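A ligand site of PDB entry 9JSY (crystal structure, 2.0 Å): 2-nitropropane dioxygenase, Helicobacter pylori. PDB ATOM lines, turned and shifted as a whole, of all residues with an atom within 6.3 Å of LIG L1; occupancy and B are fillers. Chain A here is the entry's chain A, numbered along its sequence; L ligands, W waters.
The side-chain sulfur (SG) of Cys 310 binds an iron atom (FE2) of LIG L1, at 2.3 Å.
S1 of LIG L1 lies close to N of Ile 323 (3.5 Å).
An iron atom (FE1) of LIG L1 is bound by the side-chain sulfur of Cys 302 (2.3 Å).
An iron atom (FE4) of LIG L1 is bound by the side-chain sulfur (SG) of Cys 306 (2.3 Å).
N of Asn 305 lies close to S2 of LIG L1 (3.6 Å).
The backbone NH (N) of Gly 313 lies close to a sulfur (S4) of LIG L1 (3.7 Å).
An iron atom (FE3) of LIG L1 is bound by the side-chain sulfur (SG) of Cys 322 (2.3 Å).
The backbone NH (N) of Cys 306 sits close to a sulfur (S3) of LIG L1 (3.6 Å).
The backbone carbonyl oxygen (O) of Cys 310 lies within hydrogen-bond range of the backbone NH (N) of Glu 315, at 3.1 Å.
The backbone NH (N) of Ala 324 lies close to the side-chain sulfur (SG) of Cys 322, 3.8 Å away.
O of Cys 306 is in hydrogen-bond range of N of Asn 107.
The side-chain sulfur of Cys 302 lies close to the backbone NH of Asn 305 (3.5 Å).
N of Asp 325 lies close to SG of Cys 322 (3.3 Å).
The side-chain amide nitrogen (ND2) of Asn 107 sits close to the backbone carbonyl oxygen (O) of Val 307 (3.5 Å).
The side-chain sulfur (SG) of Cys 310 lies close to the backbone NH (N) of Ala 316.
ND2 of Asn 107 is in hydrogen-bond range of O of Asn 305, 2.8 Å away.
A sulfur (S3) of LIG L1 lies close to the backbone carbonyl oxygen (O) of Val 307.
Residues that only touch LIG L1: Ala 324 (3.6 Å), Pro 276 (3.8 Å) and Ala 316 (3.9 Å).
Hydrophobic or aromatic side chains within 4 Å of LIG L1: Pro 276, Ala 316, Ile 323 and Ala 324.
Water W1 lies within hydrogen-bond range of OD1 of Asp 325 (2.8 Å), N of Val 303 (2.9 Å), N of Ser 304 (2.9 Å) and S2 of LIG L1 (3.2 Å).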
ATOM      1  N   ASN A 107     -21.512 -27.000 -31.267  1.00  0.00           N
ATOM      2  CA  ASN A 107     -20.424 -26.302 -31.926  1.00  0.00           C
ATOM      3  C   ASN A 107     -19.723 -27.245 -32.894  1.00  0.00           C
ATOM      4  O   ASN A 107     -19.671 -28.449 -32.680  1.00  0.00           O
ATOM      5  CB  ASN A 107     -19.442 -25.726 -30.892  1.00  0.00           C
ATOM      6  CG  ASN A 107     -20.020 -24.559 -30.138  1.00  0.00           C
ATOM      7  OD1 ASN A 107     -20.435 -23.569 -30.751  1.00  0.00           O
ATOM      8  ND2 ASN A 107     -20.041 -24.641 -28.812  1.00  0.00           N
ATOM      9  N   PRO A 276     -29.315 -26.457 -21.330  1.00  0.00           N
ATOM     10  CA  PRO A 276     -28.454 -25.392 -21.861  1.00  0.00           C
ATOM     11  C   PRO A 276     -28.580 -25.224 -23.361  1.00  0.00           C
ATOM     12  O   PRO A 276     -28.108 -24.217 -23.900  1.00  0.00           O
ATOM     13  CB  PRO A 276     -27.034 -25.853 -21.487  1.00  0.00           C
ATOM     14  CG  PRO A 276     -27.207 -26.907 -20.463  1.00  0.00           C
ATOM     15  CD  PRO A 276     -28.529 -27.570 -20.771  1.00  0.00           C
ATOM     16  N   ILE A 300     -20.324 -25.207 -12.388  1.00  0.00           N
ATOM     17  CA  ILE A 300     -20.334 -25.136 -13.844  1.00  0.00           C
ATOM     18  C   ILE A 300     -19.105 -24.357 -14.297  1.00  0.00           C
ATOM     19  O   ILE A 300     -18.838 -23.256 -13.793  1.00  0.00           O
ATOM     20  CB  ILE A 300     -21.652 -24.541 -14.336  1.00  0.00           C
ATOM     21  CG1 ILE A 300     -22.747 -25.605 -14.103  1.00  0.00           C
ATOM     22  CG2 ILE A 300     -21.510 -24.055 -15.799  1.00  0.00           C
ATOM     23  CD1 ILE A 300     -24.107 -25.193 -14.381  1.00  0.00           C
ATOM     24  N   ALA A 301     -18.338 -24.961 -15.191  1.00  0.00           N
ATOM     25  CA  ALA A 301     -17.113 -24.356 -15.715  1.00  0.00           C
ATOM     26  C   ALA A 301     -16.897 -24.935 -17.106  1.00  0.00           C
ATOM     27  O   ALA A 301     -16.357 -26.041 -17.234  1.00  0.00           O
ATOM     28  CB  ALA A 301     -15.925 -24.629 -14.787  1.00  0.00           C
ATOM     29  N   CYS A 302     -17.354 -24.216 -18.131  1.00  0.00           N
ATOM     30  CA  CYS A 302     -17.439 -24.780 -19.465  1.00  0.00           C
ATOM     31  C   CYS A 302     -16.053 -25.212 -19.916  1.00  0.00           C
ATOM     32  O   CYS A 302     -15.153 -24.377 -20.046  1.00  0.00           O
ATOM     33  CB  CYS A 302     -18.028 -23.766 -20.453  1.00  0.00           C
ATOM     34  SG  CYS A 302     -18.112 -24.349 -22.176  1.00  0.00           S
ATOM     35  N   VAL A 303     -15.858 -26.510 -20.109  1.00  0.00           N
ATOM     36  CA  VAL A 303     -14.613 -27.065 -20.621  1.00  0.00           C
ATOM     37  C   VAL A 303     -14.795 -27.635 -22.022  1.00  0.00           C
ATOM     38  O   VAL A 303     -14.019 -27.342 -22.932  1.00  0.00           O
ATOM     39  CB  VAL A 303     -14.029 -28.114 -19.657  1.00  0.00           C
ATOM     40  CG1 VAL A 303     -12.883 -28.877 -20.350  1.00  0.00           C
ATOM     41  CG2 VAL A 303     -13.506 -27.464 -18.356  1.00  0.00           C
ATOM     42  N   SER A 304     -15.832 -28.457 -22.233  1.00  0.00           N
ATOM     43  CA  SER A 304     -15.947 -29.060 -23.565  1.00  0.00           C
ATOM     44  C   SER A 304     -16.632 -28.153 -24.597  1.00  0.00           C
ATOM     45  O   SER A 304     -16.611 -28.486 -25.782  1.00  0.00           O
ATOM     46  CB  SER A 304     -16.672 -30.417 -23.510  1.00  0.00           C
ATOM     47  OG  SER A 304     -16.218 -31.236 -22.431  1.00  0.00           O
ATOM     48  N   ASN A 305     -17.239 -27.040 -24.195  1.00  0.00           N
ATOM     49  CA  ASN A 305     -17.873 -26.109 -25.140  1.00  0.00           C
ATOM     50  C   ASN A 305     -18.793 -26.848 -26.129  1.00  0.00           C
ATOM     51  O   ASN A 305     -18.694 -26.678 -27.344  1.00  0.00           O
ATOM     52  CB  ASN A 305     -16.817 -25.326 -25.930  1.00  0.00           C
ATOM     53  CG  ASN A 305     -17.404 -24.154 -26.658  1.00  0.00           C
ATOM     54  OD1 ASN A 305     -18.480 -23.672 -26.297  1.00  0.00           O
ATOM     55  ND2 ASN A 305     -16.767 -23.763 -27.745  1.00  0.00           N
ATOM     56  N   CYS A 306     -19.719 -27.650 -25.580  1.00  0.00           N
ATOM     57  CA  CYS A 306     -20.431 -28.613 -26.411  1.00  0.00           C
ATOM     58  C   CYS A 306     -21.425 -27.980 -27.389  1.00  0.00           C
ATOM     59  O   CYS A 306     -21.539 -28.446 -28.529  1.00  0.00           O
ATOM     60  CB  CYS A 306     -21.109 -29.664 -25.494  1.00  0.00           C
ATOM     61  SG  CYS A 306     -22.495 -29.066 -24.510  1.00  0.00           S
ATOM     62  N   VAL A 307     -22.201 -26.951 -26.992  1.00  0.00           N
ATOM     63  CA  VAL A 307     -23.284 -26.470 -27.856  1.00  0.00           C
ATOM     64  C   VAL A 307     -23.275 -24.948 -27.947  1.00  0.00           C
ATOM     65  O   VAL A 307     -22.984 -24.251 -26.967  1.00  0.00           O
ATOM     66  CB  VAL A 307     -24.674 -26.962 -27.375  1.00  0.00           C
ATOM     67  CG1 VAL A 307     -24.769 -28.491 -27.499  1.00  0.00           C
ATOM     68  CG2 VAL A 307     -24.982 -26.505 -25.955  1.00  0.00           C
ATOM     69  N   ALA A 308     -23.630 -24.422 -29.136  1.00  0.00           N
ATOM     70  CA  ALA A 308     -23.605 -22.972 -29.335  1.00  0.00           C
ATOM     71  C   ALA A 308     -24.634 -22.210 -28.493  1.00  0.00           C
ATOM     72  O   ALA A 308     -24.297 -21.136 -27.974  1.00  0.00           O
ATOM     73  CB  ALA A 308     -23.803 -22.641 -30.821  1.00  0.00           C
ATOM     74  N   CYS A 310     -25.600 -22.448 -25.550  1.00  0.00           N
ATOM     75  CA  CYS A 310     -25.278 -22.282 -24.142  1.00  0.00           C
ATOM     76  C   CYS A 310     -24.434 -21.037 -23.889  1.00  0.00           C
ATOM     77  O   CYS A 310     -24.445 -20.516 -22.764  1.00  0.00           O
ATOM     78  CB  CYS A 310     -24.560 -23.526 -23.608  1.00  0.00           C
ATOM     79  SG  CYS A 310     -24.144 -23.414 -21.816  1.00  0.00           S
ATOM     80  N   ASN A 311     -23.708 -20.556 -24.907  1.00  0.00           N
ATOM     81  CA  ASN A 311     -22.814 -19.414 -24.749  1.00  0.00           C
ATOM     82  C   ASN A 311     -21.785 -19.672 -23.659  1.00  0.00           C
ATOM     83  O   ASN A 311     -21.633 -18.888 -22.720  1.00  0.00           O
ATOM     84  CB  ASN A 311     -23.616 -18.139 -24.470  1.00  0.00           C
ATOM     85  CG  ASN A 311     -22.816 -16.892 -24.745  1.00  0.00           C
ATOM     86  OD1 ASN A 311     -21.755 -16.940 -25.388  1.00  0.00           O
ATOM     87  ND2 ASN A 311     -23.269 -15.777 -24.192  1.00  0.00           N
ATOM     88  N   ARG A 312     -21.089 -20.801 -23.768  1.00  0.00           N
ATOM     89  CA  ARG A 312     -19.955 -21.162 -22.906  1.00  0.00           C
ATOM     90  C   ARG A 312     -20.291 -21.052 -21.405  1.00  0.00           C
ATOM     91  O   ARG A 312     -19.495 -20.579 -20.588  1.00  0.00           O
ATOM     92  CB  ARG A 312     -18.708 -20.335 -23.261  1.00  0.00           C
ATOM     93  CG  ARG A 312     -18.416 -20.327 -24.797  1.00  0.00           C
ATOM     94  CD  ARG A 312     -17.148 -19.549 -25.206  1.00  0.00           C
ATOM     95  NE  ARG A 312     -16.298 -20.155 -26.235  1.00  0.00           N
ATOM     96  CZ  ARG A 312     -15.385 -21.114 -26.067  1.00  0.00           C
ATOM     97  NH1 ARG A 312     -15.238 -21.728 -24.903  1.00  0.00           N
ATOM     98  NH2 ARG A 312     -14.607 -21.454 -27.089  1.00  0.00           N
ATOM     99  N   GLY A 313     -21.467 -21.542 -21.022  1.00  0.00           N
ATOM    100  CA  GLY A 313     -21.833 -21.645 -19.620  1.00  0.00           C
ATOM    101  C   GLY A 313     -22.981 -20.751 -19.212  1.00  0.00           C
ATOM    102  O   GLY A 313     -23.556 -20.976 -18.122  1.00  0.00           O
ATOM    103  N   GLU A 314     -23.369 -19.773 -20.030  1.00  0.00           N
ATOM    104  CA  GLU A 314     -24.430 -18.859 -19.614  1.00  0.00           C
ATOM    105  C   GLU A 314     -25.710 -19.635 -19.292  1.00  0.00           C
ATOM    106  O   GLU A 314     -26.272 -19.514 -18.195  1.00  0.00           O
ATOM    107  CB  GLU A 314     -24.696 -17.806 -20.703  1.00  0.00           C
ATOM    108  CG  GLU A 314     -26.046 -17.104 -20.535  1.00  0.00           C
ATOM    109  CD  GLU A 314     -26.628 -16.485 -21.817  1.00  0.00           C
ATOM    110  OE1 GLU A 314     -25.903 -16.240 -22.811  1.00  0.00           O
ATOM    111  OE2 GLU A 314     -27.843 -16.205 -21.810  1.00  0.00           O
ATOM    112  N   GLU A 315     -26.192 -20.455 -20.229  1.00  0.00           N
ATOM    113  CA  GLU A 315     -27.451 -21.156 -19.988  1.00  0.00           C
ATOM    114  C   GLU A 315     -27.278 -22.304 -19.003  1.00  0.00           C
ATOM    115  O   GLU A 315     -28.181 -22.568 -18.209  1.00  0.00           O
ATOM    116  CB  GLU A 315     -28.056 -21.674 -21.293  1.00  0.00           C
ATOM    117  CG  GLU A 315     -28.315 -20.573 -22.330  1.00  0.00           C
ATOM    118  CD  GLU A 315     -29.359 -19.531 -21.908  1.00  0.00           C
ATOM    119  OE1 GLU A 315     -30.107 -19.774 -20.943  1.00  0.00           O
ATOM    120  OE2 GLU A 315     -29.408 -18.467 -22.554  1.00  0.00           O
ATOM    121  N   ALA A 316     -26.130 -22.982 -19.029  1.00  0.00           N
ATOM    122  CA  ALA A 316     -25.878 -24.036 -18.045  1.00  0.00           C
ATOM    123  C   ALA A 316     -26.010 -23.507 -16.619  1.00  0.00           C
ATOM    124  O   ALA A 316     -26.596 -24.161 -15.742  1.00  0.00           O
ATOM    125  CB  ALA A 316     -24.490 -24.645 -18.274  1.00  0.00           C
ATOM    126  N   TYR A 321     -27.036 -27.024 -14.559  1.00  0.00           N
ATOM    127  CA  TYR A 321     -26.177 -28.155 -14.873  1.00  0.00           C
ATOM    128  C   TYR A 321     -25.553 -27.962 -16.249  1.00  0.00           C
ATOM    129  O   TYR A 321     -26.066 -27.206 -17.088  1.00  0.00           O
ATOM    130  CB  TYR A 321     -26.969 -29.467 -14.830  1.00  0.00           C
ATOM    131  CG  TYR A 321     -28.006 -29.586 -15.930  1.00  0.00           C
ATOM    132  CD1 TYR A 321     -29.292 -29.088 -15.747  1.00  0.00           C
ATOM    133  CD2 TYR A 321     -27.702 -30.207 -17.130  1.00  0.00           C
ATOM    134  CE1 TYR A 321     -30.244 -29.195 -16.745  1.00  0.00           C
ATOM    135  CE2 TYR A 321     -28.641 -30.310 -18.152  1.00  0.00           C
ATOM    136  CZ  TYR A 321     -29.918 -29.798 -17.954  1.00  0.00           C
ATOM    137  OH  TYR A 321     -30.861 -29.901 -18.947  1.00  0.00           O
ATOM    138  N   CYS A 322     -24.449 -28.664 -16.479  1.00  0.00           N
ATOM    139  CA  CYS A 322     -23.771 -28.674 -17.763  1.00  0.00           C
ATOM    140  C   CYS A 322     -24.109 -29.993 -18.444  1.00  0.00           C
ATOM    141  O   CYS A 322     -23.873 -31.059 -17.871  1.00  0.00           O
ATOM    142  CB  CYS A 322     -22.253 -28.518 -17.575  1.00  0.00           C
ATOM    143  SG  CYS A 322     -21.202 -29.020 -18.989  1.00  0.00           S
ATOM    144  N   ILE A 323     -24.684 -29.932 -19.638  1.00  0.00           N
ATOM    145  CA  ILE A 323     -25.188 -31.180 -20.216  1.00  0.00           C
ATOM    146  C   ILE A 323     -24.046 -32.056 -20.736  1.00  0.00           C
ATOM    147  O   ILE A 323     -24.127 -33.291 -20.660  1.00  0.00           O
ATOM    148  CB  ILE A 323     -26.247 -30.865 -21.288  1.00  0.00           C
ATOM    149  CG1 ILE A 323     -26.971 -32.146 -21.727  1.00  0.00           C
ATOM    150  CG2 ILE A 323     -25.642 -30.127 -22.486  1.00  0.00           C
ATOM    151  CD1 ILE A 323     -28.261 -31.847 -22.510  1.00  0.00           C
ATOM    152  N   ALA A 324     -22.956 -31.461 -21.243  1.00  0.00           N
ATOM    153  CA  ALA A 324     -21.800 -32.278 -21.626  1.00  0.00           C
ATOM    154  C   ALA A 324     -21.250 -33.047 -20.432  1.00  0.00           C
ATOM    155  O   ALA A 324     -21.069 -34.262 -20.507  1.00  0.00           O
ATOM    156  CB  ALA A 324     -20.709 -31.392 -22.245  1.00  0.00           C
ATOM    157  N   ASP A 325     -20.963 -32.333 -19.332  1.00  0.00           N
ATOM    158  CA  ASP A 325     -20.390 -32.980 -18.138  1.00  0.00           C
ATOM    159  C   ASP A 325     -21.323 -34.057 -17.606  1.00  0.00           C
ATOM    160  O   ASP A 325     -20.885 -35.163 -17.266  1.00  0.00           O
ATOM    161  CB  ASP A 325     -20.130 -31.970 -17.027  1.00  0.00           C
ATOM    162  CG  ASP A 325     -19.082 -30.940 -17.387  1.00  0.00           C
ATOM    163  OD1 ASP A 325     -18.446 -31.038 -18.457  1.00  0.00           O
ATOM    164  OD2 ASP A 325     -18.899 -30.010 -16.568  1.00  0.00           O
HETATM  165 FE1  LIG L   1     -20.004 -25.632 -22.027  1.00  0.00          FE
HETATM  166 FE2  LIG L   1     -22.657 -25.180 -21.719  1.00  0.00          FE
HETATM  167 FE3  LIG L   1     -21.502 -27.321 -20.456  1.00  0.00          FE
HETATM  168 FE4  LIG L   1     -21.818 -27.389 -23.113  1.00  0.00          FE
HETATM  169  S1  LIG L   1     -23.490 -27.316 -21.567  1.00  0.00           S
HETATM  170  S2  LIG L   1     -19.886 -27.886 -21.976  1.00  0.00           S
HETATM  171  S3  LIG L   1     -21.493 -25.223 -23.667  1.00  0.00           S
HETATM  172  S4  LIG L   1     -21.094 -25.108 -20.058  1.00  0.00           S
HETATM  173  C1  LG2 L   2     -33.850 -35.921 -24.796  1.00  0.00           C
HETATM  174  C2  LG2 L   2     -36.421 -36.931 -25.201  1.00  0.00           C
HETATM  175  C3  LG2 L   2     -33.128 -32.303 -25.911  1.00  0.00           C
HETATM  176  C4  LG2 L   2     -32.897 -31.135 -25.174  1.00  0.00           C
HETATM  177  C5  LG2 L   2     -26.283 -31.881 -25.750  1.00  0.00           C
HETATM  178  C6  LG2 L   2     -27.305 -34.446 -25.902  1.00  0.00           C
HETATM  179  C7  LG2 L   2     -28.166 -33.351 -25.980  1.00  0.00           C
HETATM  180  C8  LG2 L   2     -30.712 -32.707 -25.787  1.00  0.00           C
HETATM  181  C9  LG2 L   2     -32.006 -33.074 -26.216  1.00  0.00           C
HETATM  182  C10 LG2 L   2     -34.489 -35.736 -26.019  1.00  0.00           C
HETATM  183  C11 LG2 L   2     -34.501 -36.617 -23.775  1.00  0.00           C
HETATM  184  C12 LG2 L   2     -35.803 -37.117 -23.965  1.00  0.00           C
HETATM  185  C13 LG2 L   2     -37.853 -37.457 -25.494  1.00  0.00           C
HETATM  186  C14 LG2 L   2     -39.503 -38.212 -27.055  1.00  0.00           C
HETATM  187  C15 LG2 L   2     -35.771 -36.250 -26.209  1.00  0.00           C
HETATM  188  C16 LG2 L   2     -31.575 -30.835 -24.773  1.00  0.00           C
HETATM  189  C17 LG2 L   2     -27.659 -32.067 -25.910  1.00  0.00           C
HETATM  190  C18 LG2 L   2     -25.438 -32.992 -25.674  1.00  0.00           C
HETATM  191  C19 LG2 L   2     -25.930 -34.270 -25.752  1.00  0.00           C
HETATM  192  N1  LG2 L   2     -29.605 -33.625 -26.147  1.00  0.00           N
HETATM  193  N2  LG2 L   2     -33.874 -35.019 -27.152  1.00  0.00           N
HETATM  194  N3  LG2 L   2     -30.532 -31.622 -25.081  1.00  0.00           N
HETATM  195  O1  LG2 L   2     -38.303 -37.482 -26.839  1.00  0.00           O
HETATM  196  O2  LG2 L   2     -38.557 -37.805 -24.612  1.00  0.00           O
HETATM  197  O3  LG2 L   2     -31.747 -34.469 -28.563  1.00  0.00           O
HETATM  198  O4  LG2 L   2     -31.359 -35.681 -26.657  1.00  0.00           O
HETATM  199  S1  LG2 L   2     -32.196 -34.606 -27.184  1.00  0.00           S
HETATM  200 CL1  LG2 L   2     -27.948 -36.094 -26.014  1.00  0.00          CL
HETATM  201 CL2  LG2 L   2     -23.685 -32.743 -25.470  1.00  0.00          CL
HETATM  202  O   HOH W   1     -17.585 -28.817 -19.947  1.00  0.00           O
